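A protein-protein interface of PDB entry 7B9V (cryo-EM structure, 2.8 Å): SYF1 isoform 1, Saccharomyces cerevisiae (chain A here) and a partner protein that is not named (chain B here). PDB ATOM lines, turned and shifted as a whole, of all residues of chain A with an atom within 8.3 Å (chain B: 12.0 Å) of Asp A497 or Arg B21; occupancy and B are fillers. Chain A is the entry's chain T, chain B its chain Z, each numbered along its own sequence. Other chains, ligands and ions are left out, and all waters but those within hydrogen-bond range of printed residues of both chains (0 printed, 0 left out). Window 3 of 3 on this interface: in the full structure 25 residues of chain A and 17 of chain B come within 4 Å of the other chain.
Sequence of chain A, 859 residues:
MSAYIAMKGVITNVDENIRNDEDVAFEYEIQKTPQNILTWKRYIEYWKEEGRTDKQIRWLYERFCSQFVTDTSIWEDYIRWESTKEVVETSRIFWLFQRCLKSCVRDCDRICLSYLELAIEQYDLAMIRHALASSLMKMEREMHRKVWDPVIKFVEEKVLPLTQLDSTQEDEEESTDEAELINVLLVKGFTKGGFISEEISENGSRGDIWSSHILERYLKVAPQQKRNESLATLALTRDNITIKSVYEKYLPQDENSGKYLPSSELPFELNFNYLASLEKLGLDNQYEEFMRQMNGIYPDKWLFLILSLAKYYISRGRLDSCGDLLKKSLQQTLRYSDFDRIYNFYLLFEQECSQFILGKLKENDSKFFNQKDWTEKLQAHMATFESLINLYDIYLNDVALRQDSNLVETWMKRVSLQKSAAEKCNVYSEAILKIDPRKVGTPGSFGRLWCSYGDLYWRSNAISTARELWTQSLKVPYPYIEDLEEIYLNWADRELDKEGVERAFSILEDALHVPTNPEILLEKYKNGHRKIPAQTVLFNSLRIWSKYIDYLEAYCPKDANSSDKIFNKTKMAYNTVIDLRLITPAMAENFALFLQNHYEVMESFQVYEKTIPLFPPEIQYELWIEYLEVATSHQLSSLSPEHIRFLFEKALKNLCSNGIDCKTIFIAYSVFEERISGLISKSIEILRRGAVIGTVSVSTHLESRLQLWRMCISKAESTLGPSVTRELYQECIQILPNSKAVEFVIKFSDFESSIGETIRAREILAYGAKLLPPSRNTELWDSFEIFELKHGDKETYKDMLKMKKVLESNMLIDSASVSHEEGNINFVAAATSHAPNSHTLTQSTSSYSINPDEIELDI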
ATOM      1  N   TRP A 458      14.387  -2.141  38.681  1.00  0.00           N
ATOM      2  CA  TRP A 458      14.301  -3.013  37.507  1.00  0.00           C
ATOM      3  C   TRP A 458      13.546  -4.315  37.744  1.00  0.00           C
ATOM      4  O   TRP A 458      12.929  -4.833  36.806  1.00  0.00           O
ATOM      5  CB  TRP A 458      15.711  -3.300  36.938  1.00  0.00           C
ATOM      6  CG  TRP A 458      15.667  -3.843  35.518  1.00  0.00           C
ATOM      7  CD1 TRP A 458      15.755  -3.147  34.357  1.00  0.00           C
ATOM      8  CD2 TRP A 458      15.574  -5.229  35.140  1.00  0.00           C
ATOM      9  NE1 TRP A 458      15.688  -3.998  33.281  1.00  0.00           N
ATOM     10  CE2 TRP A 458      15.568  -5.287  33.740  1.00  0.00           C
ATOM     11  CE3 TRP A 458      15.483  -6.430  35.840  1.00  0.00           C
ATOM     12  CZ2 TRP A 458      15.472  -6.485  33.033  1.00  0.00           C
ATOM     13  CZ3 TRP A 458      15.377  -7.630  35.146  1.00  0.00           C
ATOM     14  CH2 TRP A 458      15.378  -7.633  33.756  1.00  0.00           C
ATOM     15  N   ILE A 463      10.672  -0.841  34.370  1.00  0.00           N
ATOM     16  CA  ILE A 463      12.044  -0.984  33.822  1.00  0.00           C
ATOM     17  C   ILE A 463      12.594   0.313  33.215  1.00  0.00           C
ATOM     18  O   ILE A 463      13.831   0.582  33.287  1.00  0.00           O
ATOM     19  CB  ILE A 463      12.103  -2.238  32.878  1.00  0.00           C
ATOM     20  CG1 ILE A 463      11.953  -3.545  33.704  1.00  0.00           C
ATOM     21  CG2 ILE A 463      13.260  -2.226  31.808  1.00  0.00           C
ATOM     22  CD1 ILE A 463      11.682  -4.790  32.882  1.00  0.00           C
ATOM     23  N   TRP A 491      24.159  -4.646  33.083  1.00  0.00           N
ATOM     24  CA  TRP A 491      23.075  -4.112  32.266  1.00  0.00           C
ATOM     25  C   TRP A 491      22.859  -5.002  31.055  1.00  0.00           C
ATOM     26  O   TRP A 491      21.748  -5.485  30.828  1.00  0.00           O
ATOM     27  CB  TRP A 491      23.348  -2.651  31.869  1.00  0.00           C
ATOM     28  CG  TRP A 491      22.267  -1.925  31.004  1.00  0.00           C
ATOM     29  CD1 TRP A 491      21.040  -2.393  30.604  1.00  0.00           C
ATOM     30  CD2 TRP A 491      22.339  -0.572  30.529  1.00  0.00           C
ATOM     31  NE1 TRP A 491      20.367  -1.447  29.896  1.00  0.00           N
ATOM     32  CE2 TRP A 491      21.137  -0.319  29.834  1.00  0.00           C
ATOM     33  CE3 TRP A 491      23.290   0.431  30.616  1.00  0.00           C
ATOM     34  CZ2 TRP A 491      20.878   0.906  29.227  1.00  0.00           C
ATOM     35  CZ3 TRP A 491      23.028   1.643  30.023  1.00  0.00           C
ATOM     36  CH2 TRP A 491      21.835   1.871  29.339  1.00  0.00           C
ATOM     37  N   ALA A 492      23.932  -5.330  30.320  1.00  0.00           N
ATOM     38  CA  ALA A 492      23.775  -6.256  29.201  1.00  0.00           C
ATOM     39  C   ALA A 492      23.577  -7.726  29.589  1.00  0.00           C
ATOM     40  O   ALA A 492      23.783  -8.602  28.751  1.00  0.00           O
ATOM     41  CB  ALA A 492      24.963  -6.149  28.247  1.00  0.00           C
ATOM     42  N   ASP A 493      23.166  -8.030  30.819  1.00  0.00           N
ATOM     43  CA  ASP A 493      22.635  -9.324  31.219  1.00  0.00           C
ATOM     44  C   ASP A 493      21.206  -9.245  31.716  1.00  0.00           C
ATOM     45  O   ASP A 493      20.427 -10.172  31.474  1.00  0.00           O
ATOM     46  CB  ASP A 493      23.545  -9.939  32.298  1.00  0.00           C
ATOM     47  CG  ASP A 493      23.053 -11.290  32.795  1.00  0.00           C
ATOM     48  OD1 ASP A 493      22.202 -11.362  33.709  1.00  0.00           O
ATOM     49  OD2 ASP A 493      23.507 -12.305  32.228  1.00  0.00           O
ATOM     50  N   ARG A 494      20.856  -8.175  32.443  1.00  0.00           N
ATOM     51  CA  ARG A 494      19.445  -7.906  32.700  1.00  0.00           C
ATOM     52  C   ARG A 494      18.707  -7.629  31.400  1.00  0.00           C
ATOM     53  O   ARG A 494      17.573  -8.084  31.212  1.00  0.00           O
ATOM     54  CB  ARG A 494      19.272  -6.717  33.653  1.00  0.00           C
ATOM     55  CG  ARG A 494      19.941  -6.814  35.018  1.00  0.00           C
ATOM     56  CD  ARG A 494      19.212  -7.751  35.965  1.00  0.00           C
ATOM     57  NE  ARG A 494      19.846  -7.773  37.280  1.00  0.00           N
ATOM     58  CZ  ARG A 494      20.646  -8.731  37.725  1.00  0.00           C
ATOM     59  NH1 ARG A 494      20.935  -9.789  36.986  1.00  0.00           N
ATOM     60  NH2 ARG A 494      21.168  -8.625  38.944  1.00  0.00           N
ATOM     61  N   GLU A 495      19.336  -6.873  30.490  1.00  0.00           N
ATOM     62  CA  GLU A 495      18.684  -6.489  29.242  1.00  0.00           C
ATOM     63  C   GLU A 495      18.485  -7.666  28.294  1.00  0.00           C
ATOM     64  O   GLU A 495      17.628  -7.568  27.406  1.00  0.00           O
ATOM     65  CB  GLU A 495      19.489  -5.386  28.553  1.00  0.00           C
ATOM     66  CG  GLU A 495      18.769  -4.570  27.508  1.00  0.00           C
ATOM     67  CD  GLU A 495      17.704  -3.704  28.121  1.00  0.00           C
ATOM     68  OE1 GLU A 495      16.553  -4.165  28.294  1.00  0.00           O
ATOM     69  OE2 GLU A 495      18.043  -2.558  28.468  1.00  0.00           O
ATOM     70  N   LEU A 496      19.293  -8.737  28.446  1.00  0.00           N
ATOM     71  CA  LEU A 496      19.271  -9.894  27.545  1.00  0.00           C
ATOM     72  C   LEU A 496      17.876 -10.496  27.441  1.00  0.00           C
ATOM     73  O   LEU A 496      17.383 -10.782  26.347  1.00  0.00           O
ATOM     74  CB  LEU A 496      20.267 -10.933  28.044  1.00  0.00           C
ATOM     75  CG  LEU A 496      20.556 -12.131  27.159  1.00  0.00           C
ATOM     76  CD1 LEU A 496      21.740 -11.827  26.271  1.00  0.00           C
ATOM     77  CD2 LEU A 496      20.822 -13.354  27.980  1.00  0.00           C
ATOM     78  N   ASP A 497      17.218 -10.681  28.583  1.00  0.00           N
ATOM     79  CA  ASP A 497      15.964 -11.408  28.654  1.00  0.00           C
ATOM     80  C   ASP A 497      14.752 -10.492  28.515  1.00  0.00           C
ATOM     81  O   ASP A 497      13.640 -10.914  28.846  1.00  0.00           O
ATOM     82  CB  ASP A 497      15.877 -12.188  29.966  1.00  0.00           C
ATOM     83  CG  ASP A 497      16.915 -13.276  30.062  1.00  0.00           C
ATOM     84  OD1 ASP A 497      17.132 -13.966  29.045  1.00  0.00           O
ATOM     85  OD2 ASP A 497      17.525 -13.432  31.141  1.00  0.00           O
ATOM     86  N   LYS A 498      14.924  -9.261  28.019  1.00  0.00           N
ATOM     87  CA  LYS A 498      13.788  -8.355  27.827  1.00  0.00           C
ATOM     88  C   LYS A 498      13.766  -7.607  26.502  1.00  0.00           C
ATOM     89  O   LYS A 498      12.702  -7.095  26.138  1.00  0.00           O
ATOM     90  CB  LYS A 498      13.692  -7.319  28.963  1.00  0.00           C
ATOM     91  CG  LYS A 498      13.442  -7.887  30.363  1.00  0.00           C
ATOM     92  CD  LYS A 498      12.060  -8.515  30.499  1.00  0.00           C
ATOM     93  CE  LYS A 498      11.849  -9.080  31.896  1.00  0.00           C
ATOM     94  NZ  LYS A 498      10.515  -9.728  32.032  1.00  0.00           N
ATOM     95  N   GLU A 499      14.879  -7.496  25.767  1.00  0.00           N
ATOM     96  CA  GLU A 499      14.807  -7.074  24.373  1.00  0.00           C
ATOM     97  C   GLU A 499      15.820  -7.802  23.494  1.00  0.00           C
ATOM     98  O   GLU A 499      16.230  -7.274  22.453  1.00  0.00           O
ATOM     99  CB  GLU A 499      14.989  -5.557  24.237  1.00  0.00           C
ATOM    100  CG  GLU A 499      14.055  -4.915  23.206  1.00  0.00           C
ATOM    101  CD  GLU A 499      14.130  -3.399  23.188  1.00  0.00           C
ATOM    102  OE1 GLU A 499      13.501  -2.759  24.057  1.00  0.00           O
ATOM    103  OE2 GLU A 499      14.815  -2.847  22.301  1.00  0.00           O
ATOM    104  N   GLY A 500      16.247  -9.002  23.890  1.00  0.00           N
ATOM    105  CA  GLY A 500      17.100  -9.804  23.033  1.00  0.00           C
ATOM    106  C   GLY A 500      18.546  -9.340  22.999  1.00  0.00           C
ATOM    107  O   GLY A 500      18.921  -8.303  23.546  1.00  0.00           O
ATOM    108  N   VAL A 501      19.390 -10.170  22.372  1.00  0.00           N
ATOM    109  CA  VAL A 501      20.804  -9.830  22.185  1.00  0.00           C
ATOM    110  C   VAL A 501      21.019  -8.611  21.309  1.00  0.00           C
ATOM    111  O   VAL A 501      22.121  -8.057  21.313  1.00  0.00           O
ATOM    112  CB  VAL A 501      21.593 -11.018  21.612  1.00  0.00           C
ATOM    113  CG1 VAL A 501      21.534 -12.098  22.557  1.00  0.00           C
ATOM    114  CG2 VAL A 501      21.014 -11.485  20.283  1.00  0.00           C
ATOM    115  N   ALA A 504      21.584  -5.945  23.680  1.00  0.00           N
ATOM    116  CA  ALA A 504      22.786  -6.265  24.462  1.00  0.00           C
ATOM    117  C   ALA A 504      24.063  -5.939  23.694  1.00  0.00           C
ATOM    118  O   ALA A 504      25.058  -5.475  24.291  1.00  0.00           O
ATOM    119  CB  ALA A 504      22.768  -7.739  24.860  1.00  0.00           C
ATOM    120  N   LYS A 547      32.818 -10.943  27.160  1.00  0.00           N
ATOM    121  CA  LYS A 547      31.357 -11.035  27.139  1.00  0.00           C
ATOM    122  C   LYS A 547      30.784 -10.825  25.762  1.00  0.00           C
ATOM    123  O   LYS A 547      29.860 -11.560  25.382  1.00  0.00           O
ATOM    124  CB  LYS A 547      30.722 -10.022  28.067  1.00  0.00           C
ATOM    125  CG  LYS A 547      29.336 -10.470  28.486  1.00  0.00           C
ATOM    126  CD  LYS A 547      29.414 -11.709  29.364  1.00  0.00           C
ATOM    127  CE  LYS A 547      28.134 -11.904  30.163  1.00  0.00           C
ATOM    128  NZ  LYS A 547      28.180 -13.147  30.982  1.00  0.00           N
ATOM    129  N   TYR A 551      28.527 -13.571  23.751  1.00  0.00           N
ATOM    130  CA  TYR A 551      27.187 -13.342  23.206  1.00  0.00           C
ATOM    131  C   TYR A 551      27.162 -13.545  21.699  1.00  0.00           C
ATOM    132  O   TYR A 551      26.222 -14.154  21.168  1.00  0.00           O
ATOM    133  CB  TYR A 551      26.694 -11.929  23.526  1.00  0.00           C
ATOM    134  CG  TYR A 551      26.322 -11.618  24.959  1.00  0.00           C
ATOM    135  CD1 TYR A 551      26.307 -12.602  25.934  1.00  0.00           C
ATOM    136  CD2 TYR A 551      25.963 -10.323  25.331  1.00  0.00           C
ATOM    137  CE1 TYR A 551      25.958 -12.308  27.239  1.00  0.00           C
ATOM    138  CE2 TYR A 551      25.623 -10.027  26.630  1.00  0.00           C
ATOM    139  CZ  TYR A 551      25.617 -11.031  27.583  1.00  0.00           C
ATOM    140  OH  TYR A 551      25.278 -10.759  28.892  1.00  0.00           O
ATOM    141  N   ALA A 554      27.468 -17.109  20.677  1.00  0.00           N
ATOM    142  CA  ALA A 554      26.231 -17.832  20.919  1.00  0.00           C
ATOM    143  C   ALA A 554      25.158 -17.522  19.885  1.00  0.00           C
ATOM    144  O   ALA A 554      24.392 -18.414  19.504  1.00  0.00           O
ATOM    145  CB  ALA A 554      25.726 -17.534  22.326  1.00  0.00           C
ATOM    146  N   ASP B  12      32.547 -24.394  25.229  1.00  0.00           N
ATOM    147  CA  ASP B  12      31.526 -24.475  24.191  1.00  0.00           C
ATOM    148  C   ASP B  12      30.241 -25.064  24.742  1.00  0.00           C
ATOM    149  O   ASP B  12      29.147 -24.685  24.304  1.00  0.00           O
ATOM    150  CB  ASP B  12      32.041 -25.272  22.989  1.00  0.00           C
ATOM    151  CG  ASP B  12      31.204 -25.060  21.742  1.00  0.00           C
ATOM    152  OD1 ASP B  12      30.988 -23.892  21.355  1.00  0.00           O
ATOM    153  OD2 ASP B  12      30.758 -26.067  21.151  1.00  0.00           O
ATOM    154  N   GLN B  13      30.360 -25.998  25.695  1.00  0.00           N
ATOM    155  CA  GLN B  13      29.163 -26.501  26.358  1.00  0.00           C
ATOM    156  C   GLN B  13      28.537 -25.434  27.244  1.00  0.00           C
ATOM    157  O   GLN B  13      27.306 -25.327  27.312  1.00  0.00           O
ATOM    158  CB  GLN B  13      29.486 -27.754  27.168  1.00  0.00           C
ATOM    159  CG  GLN B  13      29.954 -28.935  26.339  1.00  0.00           C
ATOM    160  CD  GLN B  13      28.893 -29.416  25.357  1.00  0.00           C
ATOM    161  OE1 GLN B  13      27.697 -29.408  25.658  1.00  0.00           O
ATOM    162  NE2 GLN B  13      29.328 -29.838  24.177  1.00  0.00           N
ATOM    163  N   GLU B  14      29.369 -24.660  27.967  1.00  0.00           N
ATOM    164  CA  GLU B  14      28.855 -23.584  28.811  1.00  0.00           C
ATOM    165  C   GLU B  14      28.195 -22.464  28.013  1.00  0.00           C
ATOM    166  O   GLU B  14      27.419 -21.693  28.586  1.00  0.00           O
ATOM    167  CB  GLU B  14      29.973 -22.998  29.675  1.00  0.00           C
ATOM    168  CG  GLU B  14      30.630 -23.987  30.633  1.00  0.00           C
ATOM    169  CD  GLU B  14      29.676 -24.536  31.679  1.00  0.00           C
ATOM    170  OE1 GLU B  14      29.308 -23.785  32.608  1.00  0.00           O
ATOM    171  OE2 GLU B  14      29.300 -25.722  31.577  1.00  0.00           O
ATOM    172  N   LEU B  15      28.513 -22.342  26.715  1.00  0.00           N
ATOM    173  CA  LEU B  15      27.853 -21.348  25.881  1.00  0.00           C
ATOM    174  C   LEU B  15      26.388 -21.677  25.664  1.00  0.00           C
ATOM    175  O   LEU B  15      25.593 -20.759  25.430  1.00  0.00           O
ATOM    176  CB  LEU B  15      28.542 -21.220  24.526  1.00  0.00           C
ATOM    177  CG  LEU B  15      29.612 -20.150  24.344  1.00  0.00           C
ATOM    178  CD1 LEU B  15      30.265 -20.319  22.987  1.00  0.00           C
ATOM    179  CD2 LEU B  15      29.003 -18.771  24.482  1.00  0.00           C
ATOM    180  N   ASN B  16      26.033 -22.982  25.662  1.00  0.00           N
ATOM    181  CA  ASN B  16      24.654 -23.402  25.403  1.00  0.00           C
ATOM    182  C   ASN B  16      23.650 -22.854  26.406  1.00  0.00           C
ATOM    183  O   ASN B  16      22.457 -22.811  26.091  1.00  0.00           O
ATOM    184  CB  ASN B  16      24.540 -24.928  25.394  1.00  0.00           C
ATOM    185  CG  ASN B  16      24.735 -25.527  24.013  1.00  0.00           C
ATOM    186  OD1 ASN B  16      24.559 -24.849  23.004  1.00  0.00           O
ATOM    187  ND2 ASN B  16      25.072 -26.814  23.964  1.00  0.00           N
ATOM    188  N   GLN B  17      24.105 -22.520  27.625  1.00  0.00           N
ATOM    189  CA  GLN B  17      23.262 -21.839  28.597  1.00  0.00           C
ATOM    190  C   GLN B  17      22.796 -20.505  28.045  1.00  0.00           C
ATOM    191  O   GLN B  17      21.604 -20.172  28.099  1.00  0.00           O
ATOM    192  CB  GLN B  17      24.005 -21.634  29.915  1.00  0.00           C
ATOM    193  CG  GLN B  17      24.353 -22.905  30.644  1.00  0.00           C
ATOM    194  CD  GLN B  17      25.375 -22.672  31.735  1.00  0.00           C
ATOM    195  OE1 GLN B  17      25.546 -21.554  32.216  1.00  0.00           O
ATOM    196  NE2 GLN B  17      26.058 -23.736  32.138  1.00  0.00           N
ATOM    197  N   LEU B  18      23.742 -19.727  27.504  1.00  0.00           N
ATOM    198  CA  LEU B  18      23.377 -18.470  26.878  1.00  0.00           C
ATOM    199  C   LEU B  18      22.583 -18.708  25.615  1.00  0.00           C
ATOM    200  O   LEU B  18      21.563 -18.052  25.415  1.00  0.00           O
ATOM    201  CB  LEU B  18      24.624 -17.650  26.576  1.00  0.00           C
ATOM    202  CG  LEU B  18      25.434 -17.167  27.780  1.00  0.00           C
ATOM    203  CD1 LEU B  18      26.567 -18.092  28.178  1.00  0.00           C
ATOM    204  CD2 LEU B  18      25.986 -15.836  27.479  1.00  0.00           C
ATOM    205  N   ARG B  19      22.990 -19.712  24.808  1.00  0.00           N
ATOM    206  CA  ARG B  19      22.279 -20.105  23.586  1.00  0.00           C
ATOM    207  C   ARG B  19      20.833 -20.498  23.878  1.00  0.00           C
ATOM    208  O   ARG B  19      19.945 -20.280  23.047  1.00  0.00           O
ATOM    209  CB  ARG B  19      23.037 -21.230  22.876  1.00  0.00           C
ATOM    210  CG  ARG B  19      22.799 -21.321  21.364  1.00  0.00           C
ATOM    211  CD  ARG B  19      23.755 -22.300  20.681  1.00  0.00           C
ATOM    212  NE  ARG B  19      25.085 -21.731  20.464  1.00  0.00           N
ATOM    213  CZ  ARG B  19      26.186 -22.119  21.090  1.00  0.00           C
ATOM    214  NH1 ARG B  19      26.166 -23.088  21.989  1.00  0.00           N
ATOM    215  NH2 ARG B  19      27.343 -21.536  20.788  1.00  0.00           N
ATOM    216  N   ALA B  20      20.586 -21.050  25.073  1.00  0.00           N
ATOM    217  CA  ALA B  20      19.231 -21.334  25.519  1.00  0.00           C
ATOM    218  C   ALA B  20      18.512 -20.048  25.900  1.00  0.00           C
ATOM    219  O   ALA B  20      17.368 -19.828  25.486  1.00  0.00           O
ATOM    220  CB  ALA B  20      19.251 -22.311  26.694  1.00  0.00           C
ATOM    221  N   ARG B  21      19.148 -19.205  26.740  1.00  0.00           N
ATOM    222  CA  ARG B  21      18.518 -17.952  27.181  1.00  0.00           C
ATOM    223  C   ARG B  21      18.255 -16.955  26.053  1.00  0.00           C
ATOM    224  O   ARG B  21      17.441 -16.039  26.230  1.00  0.00           O
ATOM    225  CB  ARG B  21      19.382 -17.289  28.264  1.00  0.00           C
ATOM    226  CG  ARG B  21      19.523 -18.096  29.575  1.00  0.00           C
ATOM    227  CD  ARG B  21      19.839 -17.237  30.806  1.00  0.00           C
ATOM    228  NE  ARG B  21      21.100 -16.516  30.667  1.00  0.00           N
ATOM    229  CZ  ARG B  21      21.265 -15.222  30.898  1.00  0.00           C
ATOM    230  NH1 ARG B  21      20.263 -14.458  31.296  1.00  0.00           N
ATOM    231  NH2 ARG B  21      22.464 -14.680  30.708  1.00  0.00           N
ATOM    232  N   ILE B  22      18.927 -17.105  24.907  1.00  0.00           N
ATOM    233  CA  ILE B  22      18.741 -16.205  23.774  1.00  0.00           C
ATOM    234  C   ILE B  22      17.405 -16.462  23.087  1.00  0.00           C
ATOM    235  O   ILE B  22      16.796 -15.536  22.533  1.00  0.00           O
ATOM    236  CB  ILE B  22      19.994 -16.333  22.874  1.00  0.00           C
ATOM    237  CG1 ILE B  22      21.132 -15.554  23.513  1.00  0.00           C
ATOM    238  CG2 ILE B  22      19.794 -15.878  21.434  1.00  0.00           C
ATOM    239  CD1 ILE B  22      22.463 -15.810  22.911  1.00  0.00           C
ATOM    240  N   ASN B  23      16.839 -17.651  23.269  1.00  0.00           N
ATOM    241  CA  ASN B  23      15.585 -18.006  22.624  1.00  0.00           C
ATOM    242  C   ASN B  23      14.405 -17.944  23.592  1.00  0.00           C
ATOM    243  O   ASN B  23      13.933 -16.855  23.929  1.00  0.00           O
ATOM    244  CB  ASN B  23      15.700 -19.405  22.010  1.00  0.00           C
ATOM    245  CG  ASN B  23      16.822 -19.498  20.979  1.00  0.00           C
ATOM    246  OD1 ASN B  23      17.317 -18.483  20.484  1.00  0.00           O
ATOM    247  ND2 ASN B  23      17.223 -20.720  20.652  1.00  0.00           N
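OD2 of Asp A493 lies within salt-bridge range of NH2 of Arg B21, 3.0 Å away.
The side-chain carboxylate (OD2) of Asp A497 is in salt-bridge range of the guanidinium group (NH1) of Arg B21 (2.9 Å).
NH2 of Arg B21 touches CD2 of Leu A496 (3.4 Å).
Val A501 touches Ile B22.
CE1 of Tyr A551 touches CD2 of Leu B18 (3.5 Å).
NE of Arg B19 touches O of Ala A554, at 3.5 Å.
Ile B22 touches Ala A554 (CD1 to CB, 3.7 Å).
Of the 17 printed residues of chain A, 6 touch a printed residue of chain B.
Printed residues of chain A that touch a printed residue of chain B: Asp A493, Leu A496, Asp A497, Val A501, Tyr A551 and Ala A554.
Printed residues of chain B that touch a printed residue of chain A: Leu B18, Arg B19, Arg B21 and Ile B22.
Among the printed residues, Asp or Glu carboxylates within 4 Å of a Lys or Arg side-chain nitrogen of the other chain: Asp A493 with Arg B21 (3.0 Å) and Asp A497 with Arg B21 (2.9 Å).
The backbone carbonyl oxygen (O) of Ala A492 is in hydrogen-bond range of the side-chain hydroxyl (OH) of Tyr A551 (2.6 Å).
The side-chain carboxylate (OD1) of Asp A493 is in salt-bridge range of the guanidinium group (NH1) of Arg A494 (3.8 Å).
NH1 of Arg B19 is in hydrogen-bond range of OD1 of Asn B16, 2.6 Å away.
Asp A493 touches just one residue of chain B: Arg B21 (3.0 Å).
Arg A494 touches none of the printed residues of chain B.
Glu A495 touches none of the printed residues of chain B.
Leu A496 touches just one residue of chain B: Arg B21 (3.4 Å).
Asp A497 touches just one residue of chain B: Arg B21.
No residue of chain B comes within 4 Å of Lys A498.
Of the printed residues of chain B, Ala A554 touches Arg B19 and Ile B22.
Ala B20 touches none of the printed residues of chain A.
Arg B21 touches just these residues of chain A: Asp A493, Leu A496 and Asp A497.
Of the printed residues of chain A, Ile B22 touches Val A501 and Ala A554.
The nearest printed residue of chain B that does not touch Tyr A551 is Ile B22 (4.5 Å).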
